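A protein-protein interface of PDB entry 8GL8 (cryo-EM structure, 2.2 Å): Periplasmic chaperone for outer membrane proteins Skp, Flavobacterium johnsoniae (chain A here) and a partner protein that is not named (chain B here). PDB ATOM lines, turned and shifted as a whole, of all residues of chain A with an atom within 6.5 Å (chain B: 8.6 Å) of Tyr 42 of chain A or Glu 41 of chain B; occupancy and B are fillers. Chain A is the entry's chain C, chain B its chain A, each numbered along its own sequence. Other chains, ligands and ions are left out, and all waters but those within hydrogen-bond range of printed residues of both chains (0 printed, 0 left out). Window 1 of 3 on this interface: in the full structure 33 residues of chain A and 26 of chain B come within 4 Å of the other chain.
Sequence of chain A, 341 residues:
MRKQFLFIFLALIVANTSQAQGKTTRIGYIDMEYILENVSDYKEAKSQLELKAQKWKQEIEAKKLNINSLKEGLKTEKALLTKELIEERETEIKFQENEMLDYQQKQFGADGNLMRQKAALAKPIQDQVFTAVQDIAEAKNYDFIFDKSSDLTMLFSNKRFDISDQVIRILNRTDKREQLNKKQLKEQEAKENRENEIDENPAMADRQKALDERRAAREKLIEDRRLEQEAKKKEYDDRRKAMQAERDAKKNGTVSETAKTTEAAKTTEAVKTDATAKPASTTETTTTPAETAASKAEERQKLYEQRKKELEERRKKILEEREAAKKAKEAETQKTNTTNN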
ATOM      1  N   LEU A  36      24.469   3.119  10.698  1.00  0.00           N
ATOM      2  CA  LEU A  36      24.056   3.923  11.840  1.00  0.00           C
ATOM      3  C   LEU A  36      24.716   5.292  11.848  1.00  0.00           C
ATOM      4  O   LEU A  36      24.162   6.228  12.433  1.00  0.00           O
ATOM      5  CB  LEU A  36      24.362   3.184  13.142  1.00  0.00           C
ATOM      6  CG  LEU A  36      23.506   1.946  13.413  1.00  0.00           C
ATOM      7  CD1 LEU A  36      23.881   1.310  14.738  1.00  0.00           C
ATOM      8  CD2 LEU A  36      22.031   2.303  13.385  1.00  0.00           C
ATOM      9  N   GLU A  37      25.884   5.433  11.218  1.00  0.00           N
ATOM     10  CA  GLU A  37      26.477   6.756  11.063  1.00  0.00           C
ATOM     11  C   GLU A  37      25.632   7.667  10.181  1.00  0.00           C
ATOM     12  O   GLU A  37      25.802   8.889  10.230  1.00  0.00           O
ATOM     13  CB  GLU A  37      27.883   6.639  10.478  1.00  0.00           C
ATOM     14  CG  GLU A  37      28.997   6.876  11.477  1.00  0.00           C
ATOM     15  CD  GLU A  37      30.369   6.676  10.865  1.00  0.00           C
ATOM     16  OE1 GLU A  37      30.510   6.888   9.644  1.00  0.00           O
ATOM     17  OE2 GLU A  37      31.304   6.307  11.606  1.00  0.00           O
ATOM     18  N   VAL A  39      22.175   7.721  10.173  1.00  0.00           N
ATOM     19  CA  VAL A  39      20.828   7.818  10.725  1.00  0.00           C
ATOM     20  C   VAL A  39      20.859   8.845  11.847  1.00  0.00           C
ATOM     21  O   VAL A  39      21.617   8.695  12.813  1.00  0.00           O
ATOM     22  CB  VAL A  39      20.319   6.461  11.233  1.00  0.00           C
ATOM     23  CG1 VAL A  39      18.998   6.630  11.956  1.00  0.00           C
ATOM     24  CG2 VAL A  39      20.170   5.486  10.079  1.00  0.00           C
ATOM     25  N   SER A  40      20.041   9.893  11.716  1.00  0.00           N
ATOM     26  CA  SER A  40      20.000  10.936  12.736  1.00  0.00           C
ATOM     27  C   SER A  40      19.341  10.444  14.017  1.00  0.00           C
ATOM     28  O   SER A  40      19.684  10.913  15.112  1.00  0.00           O
ATOM     29  CB  SER A  40      19.266  12.162  12.200  1.00  0.00           C
ATOM     30  OG  SER A  40      18.103  11.783  11.485  1.00  0.00           O
ATOM     31  N   ASP A  41      18.392   9.513  13.900  1.00  0.00           N
ATOM     32  CA  ASP A  41      17.745   8.959  15.082  1.00  0.00           C
ATOM     33  C   ASP A  41      18.748   8.288  16.005  1.00  0.00           C
ATOM     34  O   ASP A  41      18.564   8.292  17.225  1.00  0.00           O
ATOM     35  CB  ASP A  41      16.659   7.968  14.669  1.00  0.00           C
ATOM     36  CG  ASP A  41      15.286   8.600  14.609  1.00  0.00           C
ATOM     37  OD1 ASP A  41      15.198   9.800  14.275  1.00  0.00           O
ATOM     38  OD2 ASP A  41      14.295   7.897  14.897  1.00  0.00           O
ATOM     39  N   TYR A  42      19.816   7.714  15.450  1.00  0.00           N
ATOM     40  CA  TYR A  42      20.849   7.104  16.280  1.00  0.00           C
ATOM     41  C   TYR A  42      21.534   8.147  17.156  1.00  0.00           C
ATOM     42  O   TYR A  42      21.726   7.939  18.360  1.00  0.00           O
ATOM     43  CB  TYR A  42      21.866   6.384  15.397  1.00  0.00           C
ATOM     44  CG  TYR A  42      22.832   5.511  16.157  1.00  0.00           C
ATOM     45  CD1 TYR A  42      22.390   4.389  16.840  1.00  0.00           C
ATOM     46  CD2 TYR A  42      24.187   5.805  16.187  1.00  0.00           C
ATOM     47  CE1 TYR A  42      23.269   3.587  17.535  1.00  0.00           C
ATOM     48  CE2 TYR A  42      25.073   5.010  16.879  1.00  0.00           C
ATOM     49  CZ  TYR A  42      24.609   3.902  17.551  1.00  0.00           C
ATOM     50  OH  TYR A  42      25.490   3.104  18.243  1.00  0.00           O
ATOM     51  N   LYS A  43      21.904   9.284  16.565  1.00  0.00           N
ATOM     52  CA  LYS A  43      22.529  10.352  17.339  1.00  0.00           C
ATOM     53  C   LYS A  43      21.564  10.918  18.371  1.00  0.00           C
ATOM     54  O   LYS A  43      21.960  11.221  19.504  1.00  0.00           O
ATOM     55  CB  LYS A  43      23.026  11.454  16.405  1.00  0.00           C
ATOM     56  CG  LYS A  43      24.527  11.449  16.190  1.00  0.00           C
ATOM     57  CD  LYS A  43      25.228  12.362  17.179  1.00  0.00           C
ATOM     58  CE  LYS A  43      25.222  13.803  16.698  1.00  0.00           C
ATOM     59  NZ  LYS A  43      25.648  13.913  15.277  1.00  0.00           N
ATOM     60  N   GLU A  44      20.290  11.067  17.999  1.00  0.00           N
ATOM     61  CA  GLU A  44      19.302  11.555  18.956  1.00  0.00           C
ATOM     62  C   GLU A  44      19.148  10.595  20.130  1.00  0.00           C
ATOM     63  O   GLU A  44      19.056  11.025  21.286  1.00  0.00           O
ATOM     64  CB  GLU A  44      17.962  11.777  18.259  1.00  0.00           C
ATOM     65  CG  GLU A  44      17.899  13.059  17.446  1.00  0.00           C
ATOM     66  CD  GLU A  44      16.615  13.185  16.651  1.00  0.00           C
ATOM     67  OE1 GLU A  44      15.617  12.535  17.024  1.00  0.00           O
ATOM     68  OE2 GLU A  44      16.605  13.936  15.653  1.00  0.00           O
ATOM     69  N   ALA A  45      19.119   9.289  19.854  1.00  0.00           N
ATOM     70  CA  ALA A  45      19.009   8.303  20.923  1.00  0.00           C
ATOM     71  C   ALA A  45      20.237   8.319  21.821  1.00  0.00           C
ATOM     72  O   ALA A  45      20.117   8.193  23.045  1.00  0.00           O
ATOM     73  CB  ALA A  45      18.796   6.912  20.333  1.00  0.00           C
ATOM     74  N   LYS A  46      21.426   8.465  21.235  1.00  0.00           N
ATOM     75  CA  LYS A  46      22.632   8.563  22.052  1.00  0.00           C
ATOM     76  C   LYS A  46      22.585   9.792  22.953  1.00  0.00           C
ATOM     77  O   LYS A  46      22.961   9.723  24.130  1.00  0.00           O
ATOM     78  CB  LYS A  46      23.871   8.598  21.160  1.00  0.00           C
ATOM     79  CG  LYS A  46      24.118   7.315  20.390  1.00  0.00           C
ATOM     80  CD  LYS A  46      25.312   7.448  19.463  1.00  0.00           C
ATOM     81  CE  LYS A  46      26.541   7.933  20.209  1.00  0.00           C
ATOM     82  NZ  LYS A  46      27.798   7.465  19.565  1.00  0.00           N
ATOM     83  N   SER A  47      22.115  10.922  22.419  1.00  0.00           N
ATOM     84  CA  SER A  47      22.003  12.129  23.232  1.00  0.00           C
ATOM     85  C   SER A  47      20.992  11.949  24.358  1.00  0.00           C
ATOM     86  O   SER A  47      21.229  12.388  25.490  1.00  0.00           O
ATOM     87  CB  SER A  47      21.620  13.319  22.353  1.00  0.00           C
ATOM     88  OG  SER A  47      22.771  13.918  21.785  1.00  0.00           O
ATOM     89  N   LEU A  49      20.142   9.120  25.806  1.00  0.00           N
ATOM     90  CA  LEU A  49      20.751   8.228  26.786  1.00  0.00           C
ATOM     91  C   LEU A  49      21.761   8.967  27.651  1.00  0.00           C
ATOM     92  O   LEU A  49      21.816   8.765  28.870  1.00  0.00           O
ATOM     93  CB  LEU A  49      21.412   7.051  26.074  1.00  0.00           C
ATOM     94  CG  LEU A  49      21.695   5.807  26.910  1.00  0.00           C
ATOM     95  CD1 LEU A  49      20.402   5.093  27.258  1.00  0.00           C
ATOM     96  CD2 LEU A  49      22.634   4.887  26.156  1.00  0.00           C
ATOM     97  N   LYS A 118      18.105   1.791  27.408  1.00  0.00           N
ATOM     98  CA  LYS A 118      18.839   1.515  26.178  1.00  0.00           C
ATOM     99  C   LYS A 118      17.989   0.722  25.196  1.00  0.00           C
ATOM    100  O   LYS A 118      17.956   1.033  24.000  1.00  0.00           O
ATOM    101  CB  LYS A 118      20.132   0.765  26.494  1.00  0.00           C
ATOM    102  CG  LYS A 118      21.388   1.518  26.111  1.00  0.00           C
ATOM    103  CD  LYS A 118      22.550   1.155  27.015  1.00  0.00           C
ATOM    104  CE  LYS A 118      22.805  -0.339  27.010  1.00  0.00           C
ATOM    105  NZ  LYS A 118      24.174  -0.662  27.491  1.00  0.00           N
ATOM    106  N   ILE A 125      15.054   2.518  16.166  1.00  0.00           N
ATOM    107  CA  ILE A 125      16.129   2.485  15.178  1.00  0.00           C
ATOM    108  C   ILE A 125      16.323   1.071  14.658  1.00  0.00           C
ATOM    109  O   ILE A 125      16.501   0.853  13.452  1.00  0.00           O
ATOM    110  CB  ILE A 125      17.430   3.044  15.782  1.00  0.00           C
ATOM    111  CG1 ILE A 125      17.169   4.385  16.463  1.00  0.00           C
ATOM    112  CG2 ILE A 125      18.495   3.186  14.712  1.00  0.00           C
ATOM    113  CD1 ILE A 125      18.167   4.711  17.538  1.00  0.00           C
ATOM    114  N   MET B  38      20.430  -5.289  17.373  1.00  0.00           N
ATOM    115  CA  MET B  38      21.385  -4.195  17.469  1.00  0.00           C
ATOM    116  C   MET B  38      21.065  -3.389  18.718  1.00  0.00           C
ATOM    117  O   MET B  38      19.895  -3.171  19.043  1.00  0.00           O
ATOM    118  CB  MET B  38      21.361  -3.298  16.222  1.00  0.00           C
ATOM    119  CG  MET B  38      20.068  -2.538  16.003  1.00  0.00           C
ATOM    120  SD  MET B  38      20.339  -0.866  15.390  1.00  0.00           S
ATOM    121  CE  MET B  38      20.450   0.043  16.930  1.00  0.00           C
ATOM    122  N   GLU B  39      22.106  -2.965  19.428  1.00  0.00           N
ATOM    123  CA  GLU B  39      21.939  -2.296  20.707  1.00  0.00           C
ATOM    124  C   GLU B  39      22.835  -1.071  20.783  1.00  0.00           C
ATOM    125  O   GLU B  39      23.875  -0.996  20.124  1.00  0.00           O
ATOM    126  CB  GLU B  39      22.249  -3.241  21.876  1.00  0.00           C
ATOM    127  CG  GLU B  39      23.018  -4.491  21.479  1.00  0.00           C
ATOM    128  CD  GLU B  39      24.518  -4.280  21.481  1.00  0.00           C
ATOM    129  OE1 GLU B  39      25.019  -3.552  20.599  1.00  0.00           O
ATOM    130  OE2 GLU B  39      25.198  -4.844  22.363  1.00  0.00           O
ATOM    131  N   LEU B  40      22.411  -0.106  21.592  1.00  0.00           N
ATOM    132  CA  LEU B  40      23.201   1.089  21.831  1.00  0.00           C
ATOM    133  C   LEU B  40      24.371   0.780  22.755  1.00  0.00           C
ATOM    134  O   LEU B  40      24.316  -0.137  23.579  1.00  0.00           O
ATOM    135  CB  LEU B  40      22.338   2.190  22.445  1.00  0.00           C
ATOM    136  CG  LEU B  40      21.445   2.994  21.502  1.00  0.00           C
ATOM    137  CD1 LEU B  40      20.223   3.496  22.243  1.00  0.00           C
ATOM    138  CD2 LEU B  40      22.216   4.153  20.907  1.00  0.00           C
ATOM    139  N   GLU B  41      25.438   1.555  22.609  1.00  0.00           N
ATOM    140  CA  GLU B  41      26.586   1.446  23.492  1.00  0.00           C
ATOM    141  C   GLU B  41      26.372   2.312  24.731  1.00  0.00           C
ATOM    142  O   GLU B  41      25.494   3.176  24.776  1.00  0.00           O
ATOM    143  CB  GLU B  41      27.882   1.846  22.776  1.00  0.00           C
ATOM    144  CG  GLU B  41      28.007   3.310  22.315  1.00  0.00           C
ATOM    145  CD  GLU B  41      26.788   3.860  21.594  1.00  0.00           C
ATOM    146  OE1 GLU B  41      26.532   5.076  21.713  1.00  0.00           O
ATOM    147  OE2 GLU B  41      26.101   3.088  20.889  1.00  0.00           O
ATOM    148  N   ASN B  42      27.187   2.063  25.751  1.00  0.00           N
ATOM    149  CA  ASN B  42      27.066   2.806  26.992  1.00  0.00           C
ATOM    150  C   ASN B  42      27.411   4.278  26.771  1.00  0.00           C
ATOM    151  O   ASN B  42      28.278   4.607  25.958  1.00  0.00           O
ATOM    152  CB  ASN B  42      27.978   2.215  28.061  1.00  0.00           C
ATOM    153  CG  ASN B  42      27.333   1.066  28.804  1.00  0.00           C
ATOM    154  OD1 ASN B  42      26.168   0.742  28.577  1.00  0.00           O
ATOM    155  ND2 ASN B  42      28.087   0.440  29.699  1.00  0.00           N
ATOM    156  N   PRO B  43      26.738   5.182  27.477  1.00  0.00           N
ATOM    157  CA  PRO B  43      27.058   6.608  27.364  1.00  0.00           C
ATOM    158  C   PRO B  43      28.457   6.891  27.879  1.00  0.00           C
ATOM    159  O   PRO B  43      28.994   6.122  28.689  1.00  0.00           O
ATOM    160  CB  PRO B  43      25.990   7.284  28.240  1.00  0.00           C
ATOM    161  CG  PRO B  43      25.464   6.203  29.121  1.00  0.00           C
ATOM    162  CD  PRO B  43      25.567   4.941  28.334  1.00  0.00           C
ATOM    163  N   PRO B  44      29.084   7.977  27.422  1.00  0.00           N
ATOM    164  CA  PRO B  44      30.469   8.258  27.841  1.00  0.00           C
ATOM    165  C   PRO B  44      30.629   8.455  29.337  1.00  0.00           C
ATOM    166  O   PRO B  44      31.746   8.308  29.848  1.00  0.00           O
ATOM    167  CB  PRO B  44      30.819   9.537  27.069  1.00  0.00           C
ATOM    168  CG  PRO B  44      29.845   9.588  25.939  1.00  0.00           C
ATOM    169  CD  PRO B  44      28.588   8.966  26.453  1.00  0.00           C
ATOM    170  N   ILE B  46      29.707   6.474  31.525  1.00  0.00           N
ATOM    171  CA  ILE B  46      29.932   5.152  32.096  1.00  0.00           C
ATOM    172  C   ILE B  46      31.282   4.668  31.583  1.00  0.00           C
ATOM    173  O   ILE B  46      31.415   4.263  30.425  1.00  0.00           O
ATOM    174  CB  ILE B  46      28.806   4.180  31.735  1.00  0.00           C
ATOM    175  CG1 ILE B  46      27.495   4.624  32.381  1.00  0.00           C
ATOM    176  CG2 ILE B  46      29.161   2.771  32.176  1.00  0.00           C
ATOM    177  CD1 ILE B  46      26.311   3.779  31.989  1.00  0.00           C
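OE2 of Glu 41 of chain B sits at hydrogen-bond distance from OH of Tyr 42 of chain A (2.7 Å).
NZ of Lys 46 of chain A lies within salt-bridge range of OE1 of Glu 41 of chain B, 3.5 Å away.
NZ of Lys 118 of chain A sits at hydrogen-bond distance from OD1 of Asn 42 of chain B, 2.7 Å away.
Among the printed residues, merely in contact across the chains: Tyr 42 of chain A with Leu 40 of chain B, Lys 46 of chain A with Leu 40 of chain B, Leu 49 of chain A with Glu 41 of chain B, Leu 49 of chain A with Pro 43 of chain B and Lys 118 of chain A with Leu 40 of chain B.
Tyr 42 of chain A touches just these residues of chain B: Leu 40 and Glu 41.
Glu 41 of chain B touches just these residues of chain A: Tyr 42, Lys 46 and Leu 49.
Printed residues of chain A within 4 Å of Asn 42 of chain B: Lys 118 (2.7 Å).
Of the printed residues of chain A, Leu 40 of chain B touches Tyr 42 (3.6 Å), Lys 46 (3.7 Å) and Lys 118 (3.8 Å).
Of the printed residues of chain B, Lys 46 of chain A touches Leu 40 and Glu 41.
Of the printed residues of chain A, Pro 43 of chain B touches Leu 49.
Printed residues of chain B within 4 Å of Lys 118 of chain A: Leu 40 and Asn 42.
Glu 44 of chain A touches none of the printed residues of chain B.
Lys 43 of chain A touches none of the printed residues of chain B.
The nearest residue of chain A that does not touch Glu 41 of chain B is Lys 118 of chain A (4.2 Å).
Printed residues of chain A that touch a printed residue of chain B: Tyr 42, Lys 46, Leu 49 and Lys 118.
Hydrophobic or aromatic side chains of chain A within 4 Å of the printed part of chain B: Tyr 42 and Leu 49.
Of the 8 printed residues of chain B, 4 touch a printed residue of chain A.
Hydrophobic or aromatic side chains of chain B that line the printed part of chain A: Leu 40 and Pro 43.
Along chain B the printed residues that touch a printed residue of chain A span positions 40 to 43.
Among the printed residues, Asp or Glu carboxylates within 4 Å of a Lys or Arg side-chain nitrogen of the other chain: Lys 46 of chain A with Glu 41 of chain B (3.5 Å).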
